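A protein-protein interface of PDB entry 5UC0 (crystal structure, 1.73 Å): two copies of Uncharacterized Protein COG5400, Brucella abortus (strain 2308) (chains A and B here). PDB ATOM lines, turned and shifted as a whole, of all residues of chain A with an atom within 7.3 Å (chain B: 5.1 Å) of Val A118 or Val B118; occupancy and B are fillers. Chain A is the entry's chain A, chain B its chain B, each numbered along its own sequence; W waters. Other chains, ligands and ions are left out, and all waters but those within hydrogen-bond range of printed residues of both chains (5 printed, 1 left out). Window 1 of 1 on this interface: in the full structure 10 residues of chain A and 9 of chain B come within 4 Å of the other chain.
The backbone carbonyl oxygen of Val A118 sits at hydrogen-bond distance from the backbone NH of Val B118 (2.9 Å).
Among the printed residues, merely in contact across the chains: Lys A32 with Ile B119 (3.8 Å), Gly A114 with Ala B120 (3.96 Å), Ala A116 with Val B118 (3.98 Å), Tyr A117 with Val B118 (3.3 Å), Val A118 with Ala B116 (3.9 Å), Val A118 with Tyr B117 (3.3 Å), Ile A119 with Tyr B117 (3.9 Å), Ala A120 with Ala B116 (3.96 Å) and Arg A144 with Val B147 (3.9 Å).
Ala A116 touches Val B118, and with the chains exchanged Val A118 touches Ala B116.
Val A118 touches its own counterpart, Val B118.
Ile A119 touches Tyr B117, but with the chains exchanged Tyr A117 does not touch Ile B119 (4.1 Å).
Arg A144 touches Val B147, but with the chains exchanged Val A147 does not touch Arg B144 (4.1 Å).
Of the 10 pairs that touch across the chains among the printed residues, 5 have their exchanged pair printed and touching as well.
Water W1 bridges OH of Tyr B117 and OH of Tyr A117.
Water W5 lies within hydrogen-bond range of O of Ala A116 (2.6 Å), O of Gly A114 (3.0 Å) and N of Ala B120 (3.3 Å).
Water W3 lies within hydrogen-bond range of the backbone carbonyl oxygen of Arg A144 (2.6 Å) and the backbone carbonyl oxygen of Arg B144 (3.0 Å).
Water W4 bridges the backbone NH (N) of Gly A114 and the guanidinium group (NH1) of Arg B144.
Water W2 bridges O of Ala B116 (2.6 Å) and N of Ala A120 (2.8 Å).
Hydrophobic or aromatic side chains of chain B within 4 Å of the printed part of chain A: Tyr B117, Val B118 and Ile B119.
Of the 19 printed residues of chain A, 8 touch a printed residue of chain B.
Hydrophobic or aromatic side chains of chain A that line the printed part of chain B: Tyr A117, Val A118 and Ile A119.
Printed residues of chain B within 4 Å of Ala A116: Val B118 (3.98 Å).
Printed residues of chain B within 4 Å of Val A118: Ala B116 (3.9 Å), Tyr B117 (3.3 Å) and Val B118 (2.9 Å).
Gly A121 touches none of the printed residues of chain B.
Leu A145 touches none of the printed residues of chain B.
Of the printed residues of chain A, Tyr B117 touches Val A118 (3.3 Å) and Ile A119 (3.9 Å).
Of the printed residues of chain A, Val B118 touches Ala A116, Tyr A117 and Val A118.
Of the printed residues of chain A, Ala B120 touches Gly A114.
The nearest printed residue of chain A that does not touch Val B118 is Ile A119 (5.1 Å).
The nearest printed residue of chain A that does not touch Ala B116 is Ile A119 (4.1 Å).
O of Tyr A117 sits at hydrogen-bond distance from N of Phe A124, 2.8 Å away.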
ATOM      1  N   ALA A  29      -9.768 -16.625 -35.624  1.00  0.00           N
ATOM      2  CA  ALA A  29     -10.757 -17.458 -34.948  1.00  0.00           C
ATOM      3  C   ALA A  29     -11.965 -17.703 -35.836  1.00  0.00           C
ATOM      4  O   ALA A  29     -12.478 -18.827 -35.891  1.00  0.00           O
ATOM      5  CB  ALA A  29     -11.181 -16.826 -33.616  1.00  0.00           C
ATOM      6  N   LYS A  32     -11.120 -20.148 -38.380  1.00  0.00           N
ATOM      7  CA  LYS A  32     -11.065 -21.497 -37.824  1.00  0.00           C
ATOM      8  C   LYS A  32     -12.453 -22.096 -37.671  1.00  0.00           C
ATOM      9  O   LYS A  32     -12.650 -23.286 -37.940  1.00  0.00           O
ATOM     10  CB  LYS A  32     -10.357 -21.496 -36.471  1.00  0.00           C
ATOM     11  CG  LYS A  32     -10.001 -22.895 -35.991  1.00  0.00           C
ATOM     12  CD  LYS A  32      -8.957 -23.514 -36.908  1.00  0.00           C
ATOM     13  CE  LYS A  32      -8.308 -24.742 -36.305  1.00  0.00           C
ATOM     14  NZ  LYS A  32      -7.606 -25.558 -37.356  1.00  0.00           N
ATOM     15  N   GLY A 114     -13.056 -30.775 -26.006  1.00  0.00           N
ATOM     16  CA  GLY A 114     -11.888 -30.540 -26.832  1.00  0.00           C
ATOM     17  C   GLY A 114     -12.096 -29.569 -27.966  1.00  0.00           C
ATOM     18  O   GLY A 114     -11.268 -29.530 -28.882  1.00  0.00           O
ATOM     19  N   SER A 115     -13.185 -28.795 -27.939  1.00  0.00           N
ATOM     20  CA  SER A 115     -13.495 -27.826 -28.979  1.00  0.00           C
ATOM     21  C   SER A 115     -12.934 -26.441 -28.693  1.00  0.00           C
ATOM     22  O   SER A 115     -13.040 -25.558 -29.547  1.00  0.00           O
ATOM     23  CB  SER A 115     -15.014 -27.753 -29.183  1.00  0.00           C
ATOM     24  OG  SER A 115     -15.672 -27.372 -27.989  1.00  0.00           O
ATOM     25  N   ALA A 116     -12.321 -26.239 -27.531  1.00  0.00           N
ATOM     26  CA  ALA A 116     -11.709 -24.955 -27.214  1.00  0.00           C
ATOM     27  C   ALA A 116     -10.655 -24.582 -28.246  1.00  0.00           C
ATOM     28  O   ALA A 116      -9.821 -25.405 -28.632  1.00  0.00           O
ATOM     29  CB  ALA A 116     -11.081 -25.002 -25.824  1.00  0.00           C
ATOM     30  N   TYR A 117     -10.700 -23.330 -28.692  1.00  0.00           N
ATOM     31  CA  TYR A 117      -9.693 -22.765 -29.582  1.00  0.00           C
ATOM     32  C   TYR A 117      -9.365 -21.342 -29.136  1.00  0.00           C
ATOM     33  O   TYR A 117     -10.273 -20.524 -28.956  1.00  0.00           O
ATOM     34  CB  TYR A 117     -10.185 -22.784 -31.039  1.00  0.00           C
ATOM     35  CG  TYR A 117      -9.193 -22.222 -32.030  1.00  0.00           C
ATOM     36  CD1 TYR A 117      -8.103 -22.975 -32.455  1.00  0.00           C
ATOM     37  CD2 TYR A 117      -9.348 -20.934 -32.551  1.00  0.00           C
ATOM     38  CE1 TYR A 117      -7.189 -22.459 -33.367  1.00  0.00           C
ATOM     39  CE2 TYR A 117      -8.444 -20.412 -33.461  1.00  0.00           C
ATOM     40  CZ  TYR A 117      -7.367 -21.182 -33.862  1.00  0.00           C
ATOM     41  OH  TYR A 117      -6.460 -20.676 -34.755  1.00  0.00           O
ATOM     42  N   VAL A 118      -8.076 -21.055 -28.944  1.00  0.00           N
ATOM     43  CA  VAL A 118      -7.602 -19.725 -28.568  1.00  0.00           C
ATOM     44  C   VAL A 118      -6.433 -19.337 -29.465  1.00  0.00           C
ATOM     45  O   VAL A 118      -5.476 -20.107 -29.607  1.00  0.00           O
ATOM     46  CB  VAL A 118      -7.165 -19.664 -27.094  1.00  0.00           C
ATOM     47  CG1 VAL A 118      -6.691 -18.248 -26.736  1.00  0.00           C
ATOM     48  CG2 VAL A 118      -8.299 -20.108 -26.197  1.00  0.00           C
ATOM     49  N   ILE A 119      -6.496 -18.140 -30.049  1.00  0.00           N
ATOM     50  CA  ILE A 119      -5.353 -17.585 -30.768  1.00  0.00           C
ATOM     51  C   ILE A 119      -5.413 -16.066 -30.687  1.00  0.00           C
ATOM     52  O   ILE A 119      -6.455 -15.464 -30.945  1.00  0.00           O
ATOM     53  CB  ILE A 119      -5.291 -18.070 -32.233  1.00  0.00           C
ATOM     54  CG1 ILE A 119      -4.012 -17.566 -32.907  1.00  0.00           C
ATOM     55  CG2 ILE A 119      -6.527 -17.655 -33.007  1.00  0.00           C
ATOM     56  CD1 ILE A 119      -3.837 -18.081 -34.315  1.00  0.00           C
ATOM     57  N   ALA A 120      -4.305 -15.457 -30.272  1.00  0.00           N
ATOM     58  CA  ALA A 120      -4.115 -14.008 -30.347  1.00  0.00           C
ATOM     59  C   ALA A 120      -5.197 -13.235 -29.595  1.00  0.00           C
ATOM     60  O   ALA A 120      -5.708 -12.222 -30.077  1.00  0.00           O
ATOM     61  CB  ALA A 120      -4.038 -13.551 -31.804  1.00  0.00           C
ATOM     62  N   GLY A 121      -5.546 -13.710 -28.403  1.00  0.00           N
ATOM     63  CA  GLY A 121      -6.502 -13.009 -27.572  1.00  0.00           C
ATOM     64  C   GLY A 121      -7.952 -13.186 -27.959  1.00  0.00           C
ATOM     65  O   GLY A 121      -8.804 -12.416 -27.511  1.00  0.00           O
ATOM     66  N   VAL A 122      -8.262 -14.169 -28.793  1.00  0.00           N
ATOM     67  CA  VAL A 122      -9.629 -14.473 -29.186  1.00  0.00           C
ATOM     68  C   VAL A 122      -9.818 -15.976 -29.046  1.00  0.00           C
ATOM     69  O   VAL A 122      -8.978 -16.752 -29.510  1.00  0.00           O
ATOM     70  CB  VAL A 122      -9.927 -14.011 -30.627  1.00  0.00           C
ATOM     71  CG1 VAL A 122     -11.399 -14.198 -30.959  1.00  0.00           C
ATOM     72  CG2 VAL A 122      -9.506 -12.562 -30.816  1.00  0.00           C
ATOM     73  N   GLY A 123     -10.903 -16.385 -28.395  1.00  0.00           N
ATOM     74  CA  GLY A 123     -11.123 -17.787 -28.123  1.00  0.00           C
ATOM     75  C   GLY A 123     -12.570 -18.159 -28.354  1.00  0.00           C
ATOM     76  O   GLY A 123     -13.466 -17.319 -28.275  1.00  0.00           O
ATOM     77  N   PHE A 124     -12.786 -19.438 -28.650  1.00  0.00           N
ATOM     78  CA  PHE A 124     -14.144 -19.945 -28.723  1.00  0.00           C
ATOM     79  C   PHE A 124     -14.159 -21.404 -28.314  1.00  0.00           C
ATOM     80  O   PHE A 124     -13.115 -22.039 -28.151  1.00  0.00           O
ATOM     81  CB  PHE A 124     -14.755 -19.774 -30.113  1.00  0.00           C
ATOM     82  CG  PHE A 124     -14.107 -20.605 -31.199  1.00  0.00           C
ATOM     83  CD1 PHE A 124     -14.414 -21.954 -31.353  1.00  0.00           C
ATOM     84  CD2 PHE A 124     -13.238 -20.018 -32.109  1.00  0.00           C
ATOM     85  CE1 PHE A 124     -13.843 -22.706 -32.376  1.00  0.00           C
ATOM     86  CE2 PHE A 124     -12.666 -20.757 -33.139  1.00  0.00           C
ATOM     87  CZ  PHE A 124     -12.966 -22.100 -33.271  1.00  0.00           C
ATOM     88  N   GLY A 140     -10.085 -11.233 -24.895  1.00  0.00           N
ATOM     89  CA  GLY A 140      -9.430 -10.906 -23.645  1.00  0.00           C
ATOM     90  C   GLY A 140      -9.500 -12.051 -22.669  1.00  0.00           C
ATOM     91  O   GLY A 140      -9.207 -13.206 -22.999  1.00  0.00           O
ATOM     92  N   GLY A 142     -12.212 -13.338 -21.376  1.00  0.00           N
ATOM     93  CA  GLY A 142     -13.212 -14.285 -21.835  1.00  0.00           C
ATOM     94  C   GLY A 142     -12.671 -15.261 -22.859  1.00  0.00           C
ATOM     95  O   GLY A 142     -13.056 -16.431 -22.874  1.00  0.00           O
ATOM     96  N   ALA A 143     -11.776 -14.793 -23.736  1.00  0.00           N
ATOM     97  CA  ALA A 143     -11.133 -15.689 -24.691  1.00  0.00           C
ATOM     98  C   ALA A 143     -10.536 -16.888 -23.983  1.00  0.00           C
ATOM     99  O   ALA A 143     -10.713 -18.027 -24.423  1.00  0.00           O
ATOM    100  CB  ALA A 143     -10.043 -14.960 -25.479  1.00  0.00           C
ATOM    101  N   ARG A 144      -9.846 -16.655 -22.870  1.00  0.00           N
ATOM    102  CA  ARG A 144      -9.133 -17.733 -22.202  1.00  0.00           C
ATOM    103  C   ARG A 144     -10.017 -18.497 -21.229  1.00  0.00           C
ATOM    104  O   ARG A 144      -9.869 -19.715 -21.090  1.00  0.00           O
ATOM    105  CB  ARG A 144      -7.913 -17.185 -21.472  1.00  0.00           C
ATOM    106  CG  ARG A 144      -6.851 -16.655 -22.390  1.00  0.00           C
ATOM    107  CD  ARG A 144      -5.630 -16.254 -21.584  1.00  0.00           C
ATOM    108  NE  ARG A 144      -5.990 -15.469 -20.406  1.00  0.00           N
ATOM    109  CZ  ARG A 144      -6.088 -14.147 -20.400  1.00  0.00           C
ATOM    110  NH1 ARG A 144      -5.844 -13.462 -21.505  1.00  0.00           N
ATOM    111  NH2 ARG A 144      -6.424 -13.508 -19.295  1.00  0.00           N
ATOM    112  N   LEU A 145     -10.937 -17.811 -20.560  1.00  0.00           N
ATOM    113  CA  LEU A 145     -11.767 -18.450 -19.545  1.00  0.00           C
ATOM    114  C   LEU A 145     -13.049 -19.049 -20.108  1.00  0.00           C
ATOM    115  O   LEU A 145     -13.532 -20.064 -19.591  1.00  0.00           O
ATOM    116  CB  LEU A 145     -12.114 -17.437 -18.450  1.00  0.00           C
ATOM    117  CG  LEU A 145     -10.923 -16.944 -17.632  1.00  0.00           C
ATOM    118  CD1 LEU A 145     -11.386 -16.052 -16.495  1.00  0.00           C
ATOM    119  CD2 LEU A 145     -10.144 -18.144 -17.091  1.00  0.00           C
ATOM    120  N   VAL A 147     -13.623 -20.723 -22.750  1.00  0.00           N
ATOM    121  CA  VAL A 147     -13.511 -22.012 -23.428  1.00  0.00           C
ATOM    122  C   VAL A 147     -13.790 -23.131 -22.430  1.00  0.00           C
ATOM    123  O   VAL A 147     -13.888 -24.306 -22.799  1.00  0.00           O
ATOM    124  CB  VAL A 147     -12.136 -22.170 -24.102  1.00  0.00           C
ATOM    125  CG1 VAL A 147     -11.856 -20.985 -25.011  1.00  0.00           C
ATOM    126  CG2 VAL A 147     -11.030 -22.340 -23.077  1.00  0.00           C
ATOM    127  N   ALA B 116      -1.271 -16.797 -25.462  1.00  0.00           N
ATOM    128  CA  ALA B 116      -1.857 -18.125 -25.342  1.00  0.00           C
ATOM    129  C   ALA B 116      -2.326 -18.650 -26.693  1.00  0.00           C
ATOM    130  O   ALA B 116      -2.869 -17.911 -27.518  1.00  0.00           O
ATOM    131  CB  ALA B 116      -3.027 -18.109 -24.363  1.00  0.00           C
ATOM    132  N   TYR B 117      -2.109 -19.941 -26.909  1.00  0.00           N
ATOM    133  CA  TYR B 117      -2.593 -20.644 -28.086  1.00  0.00           C
ATOM    134  C   TYR B 117      -3.157 -21.987 -27.643  1.00  0.00           C
ATOM    135  O   TYR B 117      -2.496 -22.710 -26.895  1.00  0.00           O
ATOM    136  CB  TYR B 117      -1.467 -20.835 -29.106  1.00  0.00           C
ATOM    137  CG  TYR B 117      -1.899 -21.546 -30.368  1.00  0.00           C
ATOM    138  CD1 TYR B 117      -2.742 -20.923 -31.282  1.00  0.00           C
ATOM    139  CD2 TYR B 117      -1.457 -22.842 -30.653  1.00  0.00           C
ATOM    140  CE1 TYR B 117      -3.142 -21.572 -32.440  1.00  0.00           C
ATOM    141  CE2 TYR B 117      -1.855 -23.496 -31.805  1.00  0.00           C
ATOM    142  CZ  TYR B 117      -2.695 -22.853 -32.694  1.00  0.00           C
ATOM    143  OH  TYR B 117      -3.101 -23.482 -33.843  1.00  0.00           O
ATOM    144  N   VAL B 118      -4.378 -22.309 -28.072  1.00  0.00           N
ATOM    145  CA  VAL B 118      -5.026 -23.567 -27.705  1.00  0.00           C
ATOM    146  C   VAL B 118      -5.674 -24.172 -28.939  1.00  0.00           C
ATOM    147  O   VAL B 118      -6.463 -23.505 -29.610  1.00  0.00           O
ATOM    148  CB  VAL B 118      -6.093 -23.385 -26.609  1.00  0.00           C
ATOM    149  CG1 VAL B 118      -6.675 -24.745 -26.215  1.00  0.00           C
ATOM    150  CG2 VAL B 118      -5.519 -22.659 -25.409  1.00  0.00           C
ATOM    151  N   ILE B 119      -5.376 -25.441 -29.215  1.00  0.00           N
ATOM    152  CA  ILE B 119      -5.968 -26.132 -30.358  1.00  0.00           C
ATOM    153  C   ILE B 119      -6.048 -27.620 -30.047  1.00  0.00           C
ATOM    154  O   ILE B 119      -5.060 -28.228 -29.633  1.00  0.00           O
ATOM    155  CB  ILE B 119      -5.176 -25.874 -31.656  1.00  0.00           C
ATOM    156  CG1 ILE B 119      -5.912 -26.462 -32.858  1.00  0.00           C
ATOM    157  CG2 ILE B 119      -3.770 -26.435 -31.564  1.00  0.00           C
ATOM    158  CD1 ILE B 119      -5.355 -25.991 -34.175  1.00  0.00           C
ATOM    159  N   ALA B 120      -7.242 -28.187 -30.211  1.00  0.00           N
ATOM    160  CA  ALA B 120      -7.500 -29.618 -30.084  1.00  0.00           C
ATOM    161  C   ALA B 120      -6.810 -30.227 -28.861  1.00  0.00           C
ATOM    162  O   ALA B 120      -5.962 -31.114 -28.969  1.00  0.00           O
ATOM    163  CB  ALA B 120      -7.090 -30.346 -31.362  1.00  0.00           C
ATOM    164  N   VAL B 122      -4.564 -29.198 -26.830  1.00  0.00           N
ATOM    165  CA  VAL B 122      -3.180 -28.837 -26.559  1.00  0.00           C
ATOM    166  C   VAL B 122      -3.107 -27.322 -26.433  1.00  0.00           C
ATOM    167  O   VAL B 122      -3.886 -26.598 -27.060  1.00  0.00           O
ATOM    168  CB  VAL B 122      -2.239 -29.343 -27.666  1.00  0.00           C
ATOM    169  CG1 VAL B 122      -0.792 -29.058 -27.320  1.00  0.00           C
ATOM    170  CG2 VAL B 122      -2.459 -30.820 -27.872  1.00  0.00           C
ATOM    171  N   GLY B 123      -2.189 -26.839 -25.603  1.00  0.00           N
ATOM    172  CA  GLY B 123      -2.093 -25.414 -25.374  1.00  0.00           C
ATOM    173  C   GLY B 123      -0.757 -25.037 -24.789  1.00  0.00           C
ATOM    174  O   GLY B 123      -0.147 -25.811 -24.047  1.00  0.00           O
ATOM    175  N   ALA B 143      -3.994 -27.697 -20.903  1.00  0.00           N
ATOM    176  CA  ALA B 143      -4.012 -26.891 -22.120  1.00  0.00           C
ATOM    177  C   ALA B 143      -4.855 -25.643 -21.920  1.00  0.00           C
ATOM    178  O   ALA B 143      -4.429 -24.534 -22.252  1.00  0.00           O
ATOM    179  CB  ALA B 143      -4.537 -27.706 -23.303  1.00  0.00           C
ATOM    180  N   ARG B 144      -6.056 -25.802 -21.358  1.00  0.00           N
ATOM    181  CA  ARG B 144      -6.949 -24.657 -21.227  1.00  0.00           C
ATOM    182  C   ARG B 144      -6.539 -23.760 -20.064  1.00  0.00           C
ATOM    183  O   ARG B 144      -6.495 -22.534 -20.213  1.00  0.00           O
ATOM    184  CB  ARG B 144      -8.390 -25.127 -21.058  1.00  0.00           C
ATOM    185  CG  ARG B 144      -8.889 -25.985 -22.185  1.00  0.00           C
ATOM    186  CD  ARG B 144     -10.389 -26.269 -22.059  1.00  0.00           C
ATOM    187  NE  ARG B 144     -10.747 -26.945 -20.813  1.00  0.00           N
ATOM    188  CZ  ARG B 144     -10.586 -28.247 -20.605  1.00  0.00           C
ATOM    189  NH1 ARG B 144     -10.068 -29.009 -21.556  1.00  0.00           N
ATOM    190  NH2 ARG B 144     -10.933 -28.789 -19.452  1.00  0.00           N
ATOM    191  N   VAL B 147      -2.580 -21.682 -19.780  1.00  0.00           N
ATOM    192  CA  VAL B 147      -2.281 -20.478 -20.553  1.00  0.00           C
ATOM    193  C   VAL B 147      -2.634 -19.202 -19.807  1.00  0.00           C
ATOM    194  O   VAL B 147      -2.394 -18.104 -20.321  1.00  0.00           O
ATOM    195  CB  VAL B 147      -2.993 -20.580 -21.919  1.00  0.00           C
ATOM    196  CG1 VAL B 147      -2.591 -21.873 -22.625  1.00  0.00           C
ATOM    197  CG2 VAL B 147      -4.510 -20.499 -21.774  1.00  0.00           C
HETATM  198  O   HOH W   1      -4.395 -22.170 -35.575  1.00  0.00           O
HETATM  199  O   HOH W   2      -1.939 -16.893 -29.770  1.00  0.00           O
HETATM  200  O   HOH W   3      -8.804 -20.911 -19.061  1.00  0.00           O
HETATM  201  O   HOH W   4     -12.633 -30.166 -23.503  1.00  0.00           O
HETATM  202  O   HOH W   5      -9.193 -27.680 -27.631  1.00  0.00           O
